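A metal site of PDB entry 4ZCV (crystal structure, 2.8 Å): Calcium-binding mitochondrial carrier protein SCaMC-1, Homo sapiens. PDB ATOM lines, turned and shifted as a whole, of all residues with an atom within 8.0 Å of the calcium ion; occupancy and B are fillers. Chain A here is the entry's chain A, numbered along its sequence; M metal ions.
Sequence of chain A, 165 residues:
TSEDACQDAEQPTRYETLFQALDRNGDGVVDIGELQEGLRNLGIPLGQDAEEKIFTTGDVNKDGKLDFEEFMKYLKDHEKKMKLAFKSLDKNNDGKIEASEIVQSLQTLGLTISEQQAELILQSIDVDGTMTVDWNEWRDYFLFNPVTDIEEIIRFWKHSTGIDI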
ATOM      1  N   PHE A  19      12.584   2.601  20.595  1.00  0.00           N
ATOM      2  CA  PHE A  19      12.423   2.151  21.966  1.00  0.00           C
ATOM      3  C   PHE A  19      10.996   1.684  22.239  1.00  0.00           C
ATOM      4  O   PHE A  19      10.790   0.609  22.795  1.00  0.00           O
ATOM      5  CB  PHE A  19      12.807   3.276  22.943  1.00  0.00           C
ATOM      6  CG  PHE A  19      12.787   2.862  24.379  1.00  0.00           C
ATOM      7  CD1 PHE A  19      13.851   2.168  24.935  1.00  0.00           C
ATOM      8  CD2 PHE A  19      11.697   3.172  25.186  1.00  0.00           C
ATOM      9  CE1 PHE A  19      13.836   1.783  26.259  1.00  0.00           C
ATOM     10  CE2 PHE A  19      11.673   2.787  26.514  1.00  0.00           C
ATOM     11  CZ  PHE A  19      12.748   2.092  27.049  1.00  0.00           C
ATOM     12  N   LEU A  22      10.355  -1.559  20.678  1.00  0.00           N
ATOM     13  CA  LEU A  22      10.949  -2.684  21.410  1.00  0.00           C
ATOM     14  C   LEU A  22      10.270  -2.977  22.754  1.00  0.00           C
ATOM     15  O   LEU A  22      10.152  -4.138  23.143  1.00  0.00           O
ATOM     16  CB  LEU A  22      12.440  -2.427  21.621  1.00  0.00           C
ATOM     17  CG  LEU A  22      13.275  -2.381  20.354  1.00  0.00           C
ATOM     18  CD1 LEU A  22      14.752  -2.181  20.666  1.00  0.00           C
ATOM     19  CD2 LEU A  22      13.064  -3.642  19.525  1.00  0.00           C
ATOM     20  N   ASP A  23       9.811  -1.937  23.442  1.00  0.00           N
ATOM     21  CA  ASP A  23       9.169  -2.097  24.747  1.00  0.00           C
ATOM     22  C   ASP A  23       7.754  -2.646  24.596  1.00  0.00           C
ATOM     23  O   ASP A  23       6.775  -1.894  24.614  1.00  0.00           O
ATOM     24  CB  ASP A  23       9.155  -0.760  25.502  1.00  0.00           C
ATOM     25  CG  ASP A  23       8.644  -0.888  26.917  1.00  0.00           C
ATOM     26  OD1 ASP A  23       8.659  -2.010  27.457  1.00  0.00           O
ATOM     27  OD2 ASP A  23       8.226   0.138  27.493  1.00  0.00           O
ATOM     28  N   ARG A  24       7.672  -3.960  24.463  1.00  0.00           N
ATOM     29  CA  ARG A  24       6.422  -4.624  24.138  1.00  0.00           C
ATOM     30  C   ARG A  24       5.383  -4.498  25.264  1.00  0.00           C
ATOM     31  O   ARG A  24       4.201  -4.278  24.997  1.00  0.00           O
ATOM     32  CB  ARG A  24       6.705  -6.091  23.802  1.00  0.00           C
ATOM     33  CG  ARG A  24       5.709  -6.697  22.848  1.00  0.00           C
ATOM     34  CD  ARG A  24       5.837  -8.204  22.724  1.00  0.00           C
ATOM     35  NE  ARG A  24       5.828  -8.853  24.024  1.00  0.00           N
ATOM     36  CZ  ARG A  24       4.955  -9.808  24.354  1.00  0.00           C
ATOM     37  NH1 ARG A  24       4.031 -10.187  23.481  1.00  0.00           N
ATOM     38  NH2 ARG A  24       5.007 -10.356  25.554  1.00  0.00           N
ATOM     39  N   ASN A  25       5.801  -4.659  26.513  1.00  0.00           N
ATOM     40  CA  ASN A  25       4.878  -4.588  27.642  1.00  0.00           C
ATOM     41  C   ASN A  25       4.662  -3.151  28.139  1.00  0.00           C
ATOM     42  O   ASN A  25       3.909  -2.918  29.077  1.00  0.00           O
ATOM     43  CB  ASN A  25       5.353  -5.469  28.807  1.00  0.00           C
ATOM     44  CG  ASN A  25       6.696  -5.045  29.342  1.00  0.00           C
ATOM     45  OD1 ASN A  25       7.473  -4.398  28.649  1.00  0.00           O
ATOM     46  ND2 ASN A  25       6.977  -5.416  30.578  1.00  0.00           N
ATOM     47  N   GLY A  26       5.374  -2.203  27.526  1.00  0.00           N
ATOM     48  CA  GLY A  26       5.224  -0.790  27.856  1.00  0.00           C
ATOM     49  C   GLY A  26       5.559  -0.417  29.292  1.00  0.00           C
ATOM     50  O   GLY A  26       4.877   0.414  29.894  1.00  0.00           O
ATOM     51  N   ASP A  27       6.600  -1.019  29.846  1.00  0.00           N
ATOM     52  CA  ASP A  27       6.993  -0.734  31.223  1.00  0.00           C
ATOM     53  C   ASP A  27       8.102   0.317  31.330  1.00  0.00           C
ATOM     54  O   ASP A  27       8.564   0.629  32.422  1.00  0.00           O
ATOM     55  CB  ASP A  27       7.436  -2.028  31.915  1.00  0.00           C
ATOM     56  CG  ASP A  27       8.633  -2.674  31.244  1.00  0.00           C
ATOM     57  OD1 ASP A  27       9.007  -2.247  30.128  1.00  0.00           O
ATOM     58  OD2 ASP A  27       9.197  -3.626  31.817  1.00  0.00           O
ATOM     59  N   GLY A  28       8.505   0.878  30.180  1.00  0.00           N
ATOM     60  CA  GLY A  28       9.508   1.912  30.162  1.00  0.00           C
ATOM     61  C   GLY A  28      10.942   1.404  30.046  1.00  0.00           C
ATOM     62  O   GLY A  28      11.887   2.199  29.972  1.00  0.00           O
ATOM     63  N   VAL A  29      11.109   0.089  30.049  1.00  0.00           N
ATOM     64  CA  VAL A  29      12.433  -0.503  29.864  1.00  0.00           C
ATOM     65  C   VAL A  29      12.378  -1.618  28.821  1.00  0.00           C
ATOM     66  O   VAL A  29      11.310  -2.148  28.530  1.00  0.00           O
ATOM     67  CB  VAL A  29      13.025  -1.090  31.168  1.00  0.00           C
ATOM     68  CG1 VAL A  29      13.207   0.007  32.214  1.00  0.00           C
ATOM     69  CG2 VAL A  29      12.149  -2.209  31.699  1.00  0.00           C
ATOM     70  N   VAL A  30      13.526  -1.926  28.258  1.00  0.00           N
ATOM     71  CA  VAL A  30      13.651  -3.017  27.307  1.00  0.00           C
ATOM     72  C   VAL A  30      14.458  -4.152  27.928  1.00  0.00           C
ATOM     73  O   VAL A  30      15.614  -3.948  28.300  1.00  0.00           O
ATOM     74  CB  VAL A  30      14.339  -2.553  25.995  1.00  0.00           C
ATOM     75  CG1 VAL A  30      14.724  -3.753  25.141  1.00  0.00           C
ATOM     76  CG2 VAL A  30      13.434  -1.607  25.224  1.00  0.00           C
ATOM     77  N   ASP A  31      13.844  -5.318  28.070  1.00  0.00           N
ATOM     78  CA  ASP A  31      14.562  -6.485  28.555  1.00  0.00           C
ATOM     79  C   ASP A  31      15.145  -7.269  27.371  1.00  0.00           C
ATOM     80  O   ASP A  31      14.789  -7.029  26.228  1.00  0.00           O
ATOM     81  CB  ASP A  31      13.672  -7.385  29.421  1.00  0.00           C
ATOM     82  CG  ASP A  31      12.325  -7.695  28.774  1.00  0.00           C
ATOM     83  OD1 ASP A  31      12.281  -8.527  27.843  1.00  0.00           O
ATOM     84  OD2 ASP A  31      11.314  -7.109  29.206  1.00  0.00           O
ATOM     85  N   ILE A  32      16.036  -8.209  27.669  1.00  0.00           N
ATOM     86  CA  ILE A  32      16.759  -8.939  26.629  1.00  0.00           C
ATOM     87  C   ILE A  32      15.795  -9.696  25.717  1.00  0.00           C
ATOM     88  O   ILE A  32      16.004  -9.774  24.504  1.00  0.00           O
ATOM     89  CB  ILE A  32      17.788  -9.934  27.252  1.00  0.00           C
ATOM     90  CG1 ILE A  32      18.617 -10.615  26.156  1.00  0.00           C
ATOM     91  CG2 ILE A  32      17.107 -10.963  28.146  1.00  0.00           C
ATOM     92  CD1 ILE A  32      19.416  -9.659  25.290  1.00  0.00           C
ATOM     93  N   GLU A  34      12.702  -8.770  25.040  1.00  0.00           N
ATOM     94  CA  GLU A  34      12.075  -7.782  24.173  1.00  0.00           C
ATOM     95  C   GLU A  34      13.005  -7.364  23.044  1.00  0.00           C
ATOM     96  O   GLU A  34      12.571  -7.096  21.926  1.00  0.00           O
ATOM     97  CB  GLU A  34      11.644  -6.557  24.986  1.00  0.00           C
ATOM     98  CG  GLU A  34      10.405  -6.779  25.827  1.00  0.00           C
ATOM     99  CD  GLU A  34      10.029  -5.560  26.635  1.00  0.00           C
ATOM    100  OE1 GLU A  34      10.893  -4.668  26.779  1.00  0.00           O
ATOM    101  OE2 GLU A  34       8.882  -5.491  27.125  1.00  0.00           O
ATOM    102  N   LEU A  35      14.305  -7.333  23.331  1.00  0.00           N
ATOM    103  CA  LEU A  35      15.265  -6.987  22.297  1.00  0.00           C
ATOM    104  C   LEU A  35      15.302  -8.073  21.232  1.00  0.00           C
ATOM    105  O   LEU A  35      15.294  -7.786  20.034  1.00  0.00           O
ATOM    106  CB  LEU A  35      16.647  -6.770  22.906  1.00  0.00           C
ATOM    107  CG  LEU A  35      17.726  -6.313  21.918  1.00  0.00           C
ATOM    108  CD1 LEU A  35      17.353  -4.945  21.368  1.00  0.00           C
ATOM    109  CD2 LEU A  35      19.082  -6.277  22.588  1.00  0.00           C
ATOM    110  N   LYS A  65      18.365  -4.349  32.643  1.00  0.00           N
ATOM    111  CA  LYS A  65      17.330  -3.690  31.853  1.00  0.00           C
ATOM    112  C   LYS A  65      17.926  -2.536  31.071  1.00  0.00           C
ATOM    113  O   LYS A  65      18.950  -1.972  31.466  1.00  0.00           O
ATOM    114  CB  LYS A  65      16.200  -3.177  32.749  1.00  0.00           C
ATOM    115  CG  LYS A  65      15.587  -4.223  33.680  1.00  0.00           C
ATOM    116  CD  LYS A  65      14.558  -3.592  34.607  1.00  0.00           C
ATOM    117  CE  LYS A  65      14.373  -4.425  35.865  1.00  0.00           C
ATOM    118  NZ  LYS A  65      13.488  -3.765  36.864  1.00  0.00           N
ATOM    119  N   LEU A  66      17.311  -2.201  29.936  1.00  0.00           N
ATOM    120  CA  LEU A  66      17.706  -1.021  29.185  1.00  0.00           C
ATOM    121  C   LEU A  66      16.606   0.045  29.265  1.00  0.00           C
ATOM    122  O   LEU A  66      15.559  -0.080  28.638  1.00  0.00           O
ATOM    123  CB  LEU A  66      17.976  -1.375  27.722  1.00  0.00           C
ATOM    124  CG  LEU A  66      19.277  -2.105  27.397  1.00  0.00           C
ATOM    125  CD1 LEU A  66      19.379  -2.373  25.901  1.00  0.00           C
ATOM    126  CD2 LEU A  66      20.474  -1.304  27.889  1.00  0.00           C
HETATM  127 CA    CA M   1       9.636  -3.751  28.515  1.00  0.00          CA
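The side-chain carboxylate (OD1) of Asp 23 sits close to the backbone NH (N) of Gly 26, at 3.3 Å. The side-chain carboxylate of Asp 23 sits at hydrogen-bond distance from the backbone NH of Gly 28 (2.8 Å). The backbone NH of Glu 34 is in hydrogen-bond range of the side-chain carboxylate of Asp 31. The backbone NH (N) of Arg 24 sits close to the side-chain carboxylate (OE2) of Glu 34 (3.3 Å).
Asp 31 touches the calcium ion (OD2 to CA, 3.8 Å).
OD1 of Asp 23 is bound to the calcium ion (2.3 Å). The calcium ion is bound by the side-chain amide oxygen (OD1) of Asn 25 (2.3 Å). The side-chain carboxylate (OD1) of Asp 27 is bound to the calcium ion (2.3 Å). O of Val 29 is bound to the calcium ion (2.3 Å). The calcium ion is bound by OE1 of Glu 34, at 2.3 Å. The side-chain carboxylate (OE2) of Glu 34 binds the calcium ion.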
